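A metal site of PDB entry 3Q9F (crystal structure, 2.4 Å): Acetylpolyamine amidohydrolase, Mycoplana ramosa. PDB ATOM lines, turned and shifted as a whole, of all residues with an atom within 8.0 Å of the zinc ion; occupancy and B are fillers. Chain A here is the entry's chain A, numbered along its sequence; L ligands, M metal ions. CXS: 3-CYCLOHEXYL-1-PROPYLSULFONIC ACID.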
ATOM      1  N   ARG A  32      17.936  -9.899  13.588  1.00  0.00           N
ATOM      2  CA  ARG A  32      18.287  -8.511  13.880  1.00  0.00           C
ATOM      3  C   ARG A  32      19.265  -8.488  15.051  1.00  0.00           C
ATOM      4  O   ARG A  32      20.334  -7.854  14.992  1.00  0.00           O
ATOM      5  CB  ARG A  32      17.044  -7.673  14.226  1.00  0.00           C
ATOM      6  CG  ARG A  32      16.117  -7.405  13.054  1.00  0.00           C
ATOM      7  CD  ARG A  32      14.885  -6.632  13.500  1.00  0.00           C
ATOM      8  NE  ARG A  32      15.227  -5.312  14.004  1.00  0.00           N
ATOM      9  CZ  ARG A  32      15.190  -4.943  15.287  1.00  0.00           C
ATOM     10  NH1 ARG A  32      14.804  -5.791  16.220  1.00  0.00           N
ATOM     11  NH2 ARG A  32      15.555  -3.719  15.633  1.00  0.00           N
ATOM     12  N   PRO A 156      11.513  -5.260  21.180  1.00  0.00           N
ATOM     13  CA  PRO A 156      11.653  -3.878  21.613  1.00  0.00           C
ATOM     14  C   PRO A 156      10.520  -3.507  22.533  1.00  0.00           C
ATOM     15  O   PRO A 156       9.668  -4.344  22.828  1.00  0.00           O
ATOM     16  CB  PRO A 156      11.621  -3.110  20.301  1.00  0.00           C
ATOM     17  CG  PRO A 156      10.642  -3.889  19.503  1.00  0.00           C
ATOM     18  CD  PRO A 156      11.048  -5.333  19.782  1.00  0.00           C
ATOM     19  N   HIS A 158       9.430   0.455  23.148  1.00  0.00           N
ATOM     20  CA  HIS A 158       8.852   1.785  23.146  1.00  0.00           C
ATOM     21  C   HIS A 158       7.429   1.997  22.586  1.00  0.00           C
ATOM     22  O   HIS A 158       6.880   3.100  22.687  1.00  0.00           O
ATOM     23  CB  HIS A 158       9.824   2.791  22.523  1.00  0.00           C
ATOM     24  CG  HIS A 158       9.890   2.767  21.036  1.00  0.00           C
ATOM     25  ND1 HIS A 158      10.218   3.872  20.284  1.00  0.00           N
ATOM     26  CD2 HIS A 158       9.668   1.763  20.154  1.00  0.00           C
ATOM     27  CE1 HIS A 158      10.191   3.560  18.998  1.00  0.00           C
ATOM     28  NE2 HIS A 158       9.864   2.288  18.892  1.00  0.00           N
ATOM     29  N   HIS A 159       6.810   0.969  22.002  1.00  0.00           N
ATOM     30  CA  HIS A 159       5.451   1.131  21.498  1.00  0.00           C
ATOM     31  C   HIS A 159       4.444   0.543  22.484  1.00  0.00           C
ATOM     32  O   HIS A 159       3.228   0.616  22.261  1.00  0.00           O
ATOM     33  CB  HIS A 159       5.280   0.468  20.120  1.00  0.00           C
ATOM     34  CG  HIS A 159       5.898   1.247  19.009  1.00  0.00           C
ATOM     35  ND1 HIS A 159       5.589   2.570  18.756  1.00  0.00           N
ATOM     36  CD2 HIS A 159       6.843   0.911  18.095  1.00  0.00           C
ATOM     37  CE1 HIS A 159       6.321   3.012  17.751  1.00  0.00           C
ATOM     38  NE2 HIS A 159       7.087   2.019  17.325  1.00  0.00           N
ATOM     39  N   GLY A 167       3.227  -2.341  17.722  1.00  0.00           N
ATOM     40  CA  GLY A 167       4.497  -1.968  17.114  1.00  0.00           C
ATOM     41  C   GLY A 167       5.649  -2.907  17.437  1.00  0.00           C
ATOM     42  O   GLY A 167       6.781  -2.431  17.545  1.00  0.00           O
ATOM     43  N   TYR A 168       5.353  -4.199  17.595  1.00  0.00           N
ATOM     44  CA  TYR A 168       6.344  -5.243  17.878  1.00  0.00           C
ATOM     45  C   TYR A 168       6.794  -5.216  19.339  1.00  0.00           C
ATOM     46  O   TYR A 168       7.728  -5.916  19.732  1.00  0.00           O
ATOM     47  CB  TYR A 168       7.588  -5.078  16.983  1.00  0.00           C
ATOM     48  CG  TYR A 168       7.314  -4.793  15.513  1.00  0.00           C
ATOM     49  CD1 TYR A 168       6.125  -5.241  14.910  1.00  0.00           C
ATOM     50  CD2 TYR A 168       8.266  -4.130  14.724  1.00  0.00           C
ATOM     51  CE1 TYR A 168       5.895  -5.039  13.559  1.00  0.00           C
ATOM     52  CE2 TYR A 168       8.054  -3.920  13.359  1.00  0.00           C
ATOM     53  CZ  TYR A 168       6.865  -4.376  12.786  1.00  0.00           C
ATOM     54  OH  TYR A 168       6.649  -4.199  11.426  1.00  0.00           O
ATOM     55  N   ASP A 193      14.292   9.178  23.022  1.00  0.00           N
ATOM     56  CA  ASP A 193      13.932   8.217  21.970  1.00  0.00           C
ATOM     57  C   ASP A 193      14.339   8.703  20.572  1.00  0.00           C
ATOM     58  O   ASP A 193      13.677   9.559  19.976  1.00  0.00           O
ATOM     59  CB  ASP A 193      12.421   7.956  22.033  1.00  0.00           C
ATOM     60  CG  ASP A 193      11.984   6.792  21.180  1.00  0.00           C
ATOM     61  OD1 ASP A 193      12.529   6.643  20.050  1.00  0.00           O
ATOM     62  OD2 ASP A 193      11.104   6.018  21.603  1.00  0.00           O
ATOM     63  N   VAL A 194      15.414   8.126  20.027  1.00  0.00           N
ATOM     64  CA  VAL A 194      15.924   8.517  18.713  1.00  0.00           C
ATOM     65  C   VAL A 194      15.459   7.597  17.579  1.00  0.00           C
ATOM     66  O   VAL A 194      15.758   7.797  16.398  1.00  0.00           O
ATOM     67  CB  VAL A 194      17.482   8.597  18.724  1.00  0.00           C
ATOM     68  CG1 VAL A 194      17.916   9.658  19.710  1.00  0.00           C
ATOM     69  CG2 VAL A 194      18.081   7.249  19.073  1.00  0.00           C
ATOM     70  N   ASP A 195      14.714   6.565  17.955  1.00  0.00           N
ATOM     71  CA  ASP A 195      14.137   5.627  16.993  1.00  0.00           C
ATOM     72  C   ASP A 195      13.311   6.487  16.010  1.00  0.00           C
ATOM     73  O   ASP A 195      12.705   7.478  16.427  1.00  0.00           O
ATOM     74  CB  ASP A 195      13.223   4.659  17.758  1.00  0.00           C
ATOM     75  CG  ASP A 195      12.611   3.613  16.874  1.00  0.00           C
ATOM     76  OD1 ASP A 195      11.772   3.998  16.028  1.00  0.00           O
ATOM     77  OD2 ASP A 195      12.971   2.412  17.057  1.00  0.00           O
ATOM     78  N   PHE A 196      13.285   6.130  14.729  1.00  0.00           N
ATOM     79  CA  PHE A 196      12.525   6.911  13.746  1.00  0.00           C
ATOM     80  C   PHE A 196      11.083   7.128  14.131  1.00  0.00           C
ATOM     81  O   PHE A 196      10.540   8.192  13.854  1.00  0.00           O
ATOM     82  CB  PHE A 196      12.553   6.240  12.370  1.00  0.00           C
ATOM     83  CG  PHE A 196      11.681   6.920  11.344  1.00  0.00           C
ATOM     84  CD1 PHE A 196      12.083   8.108  10.747  1.00  0.00           C
ATOM     85  CD2 PHE A 196      10.446   6.373  10.998  1.00  0.00           C
ATOM     86  CE1 PHE A 196      11.269   8.766   9.802  1.00  0.00           C
ATOM     87  CE2 PHE A 196       9.622   7.011  10.057  1.00  0.00           C
ATOM     88  CZ  PHE A 196      10.039   8.214   9.467  1.00  0.00           C
ATOM     89  N   HIS A 197      10.451   6.134  14.733  1.00  0.00           N
ATOM     90  CA  HIS A 197       9.055   6.286  15.134  1.00  0.00           C
ATOM     91  C   HIS A 197       8.933   6.879  16.519  1.00  0.00           C
ATOM     92  O   HIS A 197       9.812   6.734  17.363  1.00  0.00           O
ATOM     93  CB  HIS A 197       8.337   4.948  15.151  1.00  0.00           C
ATOM     94  CG  HIS A 197       8.295   4.255  13.833  1.00  0.00           C
ATOM     95  ND1 HIS A 197       9.301   3.432  13.387  1.00  0.00           N
ATOM     96  CD2 HIS A 197       7.386   4.313  12.827  1.00  0.00           C
ATOM     97  CE1 HIS A 197       9.027   3.016  12.171  1.00  0.00           C
ATOM     98  NE2 HIS A 197       7.867   3.530  11.801  1.00  0.00           N
ATOM     99  N   HIS A 198       7.795   7.526  16.743  1.00  0.00           N
ATOM    100  CA  HIS A 198       7.536   8.131  18.030  1.00  0.00           C
ATOM    101  C   HIS A 198       7.339   6.994  19.036  1.00  0.00           C
ATOM    102  O   HIS A 198       6.801   5.942  18.700  1.00  0.00           O
ATOM    103  CB  HIS A 198       6.279   9.000  17.938  1.00  0.00           C
ATOM    104  CG  HIS A 198       5.780   9.450  19.269  1.00  0.00           C
ATOM    105  ND1 HIS A 198       4.573   9.036  19.785  1.00  0.00           N
ATOM    106  CD2 HIS A 198       6.316  10.279  20.200  1.00  0.00           C
ATOM    107  CE1 HIS A 198       4.385   9.588  20.971  1.00  0.00           C
ATOM    108  NE2 HIS A 198       5.422  10.351  21.240  1.00  0.00           N
ATOM    109  N   PHE A 225       3.770   5.907  11.314  1.00  0.00           N
ATOM    110  CA  PHE A 225       3.395   5.085  12.458  1.00  0.00           C
ATOM    111  C   PHE A 225       4.029   5.760  13.687  1.00  0.00           C
ATOM    112  O   PHE A 225       5.148   6.286  13.596  1.00  0.00           O
ATOM    113  CB  PHE A 225       3.995   3.682  12.296  1.00  0.00           C
ATOM    114  CG  PHE A 225       3.600   2.721  13.369  1.00  0.00           C
ATOM    115  CD1 PHE A 225       2.429   1.976  13.248  1.00  0.00           C
ATOM    116  CD2 PHE A 225       4.395   2.529  14.487  1.00  0.00           C
ATOM    117  CE1 PHE A 225       2.079   1.051  14.213  1.00  0.00           C
ATOM    118  CE2 PHE A 225       4.042   1.602  15.461  1.00  0.00           C
ATOM    119  CZ  PHE A 225       2.877   0.861  15.322  1.00  0.00           C
ATOM    120  N   LEU A 281      17.273   3.513  21.528  1.00  0.00           N
ATOM    121  CA  LEU A 281      17.966   3.535  20.263  1.00  0.00           C
ATOM    122  C   LEU A 281      17.366   2.704  19.149  1.00  0.00           C
ATOM    123  O   LEU A 281      17.268   1.480  19.236  1.00  0.00           O
ATOM    124  CB  LEU A 281      19.421   3.110  20.480  1.00  0.00           C
ATOM    125  CG  LEU A 281      20.238   2.830  19.221  1.00  0.00           C
ATOM    126  CD1 LEU A 281      20.353   4.078  18.364  1.00  0.00           C
ATOM    127  CD2 LEU A 281      21.630   2.338  19.641  1.00  0.00           C
ATOM    128  N   GLY A 282      16.947   3.399  18.099  1.00  0.00           N
ATOM    129  CA  GLY A 282      16.406   2.747  16.937  1.00  0.00           C
ATOM    130  C   GLY A 282      17.283   3.297  15.827  1.00  0.00           C
ATOM    131  O   GLY A 282      17.634   4.473  15.851  1.00  0.00           O
ATOM    132  N   VAL A 283      17.685   2.457  14.872  1.00  0.00           N
ATOM    133  CA  VAL A 283      18.505   2.967  13.779  1.00  0.00           C
ATOM    134  C   VAL A 283      17.733   2.949  12.477  1.00  0.00           C
ATOM    135  O   VAL A 283      18.319   2.969  11.398  1.00  0.00           O
ATOM    136  CB  VAL A 283      19.832   2.162  13.595  1.00  0.00           C
ATOM    137  CG1 VAL A 283      20.736   2.368  14.801  1.00  0.00           C
ATOM    138  CG2 VAL A 283      19.534   0.689  13.382  1.00  0.00           C
ATOM    139  N   ASP A 284      16.408   2.904  12.583  1.00  0.00           N
ATOM    140  CA  ASP A 284      15.592   2.926  11.389  1.00  0.00           C
ATOM    141  C   ASP A 284      15.511   4.341  10.822  1.00  0.00           C
ATOM    142  O   ASP A 284      14.740   4.610   9.906  1.00  0.00           O
ATOM    143  CB  ASP A 284      14.187   2.332  11.629  1.00  0.00           C
ATOM    144  CG  ASP A 284      13.593   2.681  12.975  1.00  0.00           C
ATOM    145  OD1 ASP A 284      14.318   3.122  13.900  1.00  0.00           O
ATOM    146  OD2 ASP A 284      12.370   2.494  13.137  1.00  0.00           O
ATOM    147  N   THR A 285      16.321   5.244  11.367  1.00  0.00           N
ATOM    148  CA  THR A 285      16.370   6.612  10.870  1.00  0.00           C
ATOM    149  C   THR A 285      17.335   6.663   9.691  1.00  0.00           C
ATOM    150  O   THR A 285      17.398   7.649   8.968  1.00  0.00           O
ATOM    151  CB  THR A 285      16.890   7.594  11.947  1.00  0.00           C
ATOM    152  OG1 THR A 285      18.113   7.083  12.500  1.00  0.00           O
ATOM    153  CG2 THR A 285      15.865   7.749  13.063  1.00  0.00           C
ATOM    154  N   ASP A 289      17.247   2.617   5.295  1.00  0.00           N
ATOM    155  CA  ASP A 289      16.198   1.831   5.904  1.00  0.00           C
ATOM    156  C   ASP A 289      14.939   2.070   5.073  1.00  0.00           C
ATOM    157  O   ASP A 289      14.596   3.218   4.781  1.00  0.00           O
ATOM    158  CB  ASP A 289      15.970   2.233   7.363  1.00  0.00           C
ATOM    159  CG  ASP A 289      15.062   1.259   8.098  1.00  0.00           C
ATOM    160  OD1 ASP A 289      13.880   1.150   7.698  1.00  0.00           O
ATOM    161  OD2 ASP A 289      15.517   0.612   9.050  1.00  0.00           O
ATOM    162  N   ILE A 291      11.622   1.648   5.776  1.00  0.00           N
ATOM    163  CA  ILE A 291      10.430   2.198   6.415  1.00  0.00           C
ATOM    164  C   ILE A 291      10.448   3.666   6.819  1.00  0.00           C
ATOM    165  O   ILE A 291       9.396   4.225   7.123  1.00  0.00           O
ATOM    166  CB  ILE A 291      10.047   1.355   7.638  1.00  0.00           C
ATOM    167  CG1 ILE A 291      11.165   1.408   8.679  1.00  0.00           C
ATOM    168  CG2 ILE A 291       9.774  -0.090   7.214  1.00  0.00           C
ATOM    169  CD1 ILE A 291      10.874   0.619   9.942  1.00  0.00           C
ATOM    170  N   SER A 292      11.613   4.295   6.813  1.00  0.00           N
ATOM    171  CA  SER A 292      11.670   5.688   7.198  1.00  0.00           C
ATOM    172  C   SER A 292      11.924   6.636   6.043  1.00  0.00           C
ATOM    173  O   SER A 292      12.312   6.213   4.957  1.00  0.00           O
ATOM    174  CB  SER A 292      12.751   5.893   8.251  1.00  0.00           C
ATOM    175  OG  SER A 292      14.041   6.021   7.664  1.00  0.00           O
ATOM    176  N   GLU A 320      15.910  -0.615  20.316  1.00  0.00           N
ATOM    177  CA  GLU A 320      14.519  -0.528  19.886  1.00  0.00           C
ATOM    178  C   GLU A 320      14.402  -1.068  18.470  1.00  0.00           C
ATOM    179  O   GLU A 320      14.814  -2.195  18.169  1.00  0.00           O
ATOM    180  CB  GLU A 320      14.015   0.909  19.915  1.00  0.00           C
ATOM    181  CG  GLU A 320      13.832   1.515  21.293  1.00  0.00           C
ATOM    182  CD  GLU A 320      12.818   0.772  22.134  1.00  0.00           C
ATOM    183  OE1 GLU A 320      11.960   0.072  21.561  1.00  0.00           O
ATOM    184  OE2 GLU A 320      12.856   0.905  23.374  1.00  0.00           O
ATOM    185  N   GLY A 321      13.851  -0.239  17.588  1.00  0.00           N
ATOM    186  CA  GLY A 321      13.654  -0.613  16.202  1.00  0.00           C
ATOM    187  C   GLY A 321      14.833  -0.498  15.256  1.00  0.00           C
ATOM    188  O   GLY A 321      15.966  -0.209  15.634  1.00  0.00           O
ATOM    189  N   GLY A 322      14.532  -0.710  13.977  1.00  0.00           N
ATOM    190  CA  GLY A 322      15.538  -0.658  12.940  1.00  0.00           C
ATOM    191  C   GLY A 322      15.335  -1.861  12.033  1.00  0.00           C
ATOM    192  O   GLY A 322      15.532  -3.011  12.446  1.00  0.00           O
ATOM    193  N   TYR A 323      14.925  -1.590  10.792  1.00  0.00           N
ATOM    194  CA  TYR A 323      14.688  -2.638   9.812  1.00  0.00           C
ATOM    195  C   TYR A 323      15.927  -3.504   9.684  1.00  0.00           C
ATOM    196  O   TYR A 323      17.051  -3.033   9.896  1.00  0.00           O
ATOM    197  CB  TYR A 323      14.363  -2.023   8.450  1.00  0.00           C
ATOM    198  CG  TYR A 323      13.767  -3.008   7.485  1.00  0.00           C
ATOM    199  CD1 TYR A 323      12.390  -3.242   7.470  1.00  0.00           C
ATOM    200  CD2 TYR A 323      14.577  -3.731   6.593  1.00  0.00           C
ATOM    201  CE1 TYR A 323      11.824  -4.169   6.609  1.00  0.00           C
ATOM    202  CE2 TYR A 323      14.024  -4.668   5.714  1.00  0.00           C
ATOM    203  CZ  TYR A 323      12.647  -4.879   5.734  1.00  0.00           C
ATOM    204  OH  TYR A 323      12.070  -5.803   4.881  1.00  0.00           O
HETATM  205  S   CXS L   1       9.667   0.179  15.518  1.00  0.00           S
HETATM  206  O1  CXS L   1       9.534   1.656  15.659  1.00  0.00           O
HETATM  207  O2  CXS L   1      10.032  -0.525  16.751  1.00  0.00           O
HETATM  208  O3  CXS L   1      10.683  -0.095  14.487  1.00  0.00           O
HETATM  209  C1  CXS L   1       8.064  -0.299  15.142  1.00  0.00           C
HETATM  210  C2  CXS L   1       7.511   0.357  13.858  1.00  0.00           C
HETATM  211  C3  CXS L   1       6.278  -0.402  13.362  1.00  0.00           C
HETATM  212  N   CXS L   1       6.345  -0.942  11.977  1.00  0.00           N
HETATM  213  C4  CXS L   1       5.345  -0.706  10.934  1.00  0.00           C
HETATM  214  C5  CXS L   1       5.550   0.631  10.186  1.00  0.00           C
HETATM  215  C6  CXS L   1       4.484   0.770   9.064  1.00  0.00           C
HETATM  216  C7  CXS L   1       3.054   0.792   9.583  1.00  0.00           C
HETATM  217  C8  CXS L   1       2.781  -0.506  10.356  1.00  0.00           C
HETATM  218  C9  CXS L   1       3.858  -0.732  11.459  1.00  0.00           C
HETATM  219 ZN    ZN M   1      11.224   2.478  14.665  1.00  0.00          ZN
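OD1 of Asp 284 sits at hydrogen-bond distance from N of Phe 196, 3.3 Å away. The backbone NH of Gly 321 lies within hydrogen-bond range of the side-chain carboxylate of Asp 195 (2.8 Å). OG of Ser 292 is in hydrogen-bond range of O of Asp 284 (2.7 Å). N of Asp 195 sits at hydrogen-bond distance from OD1 of Asp 193, at 3.0 Å.
Of the 25 residues printed, 3 come within 4 Å of the zinc ion.
The zinc ion is bound by OD2 of Asp 284 (1.9 Å), OD1 of Asp 195 (2.1 Å), O1 of the ligand (2.1 Å) and ND1 of His 197 (2.5 Å). Slightly farther from the zinc ion lies an oxygen (O3) of the ligand (2.6 Å).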
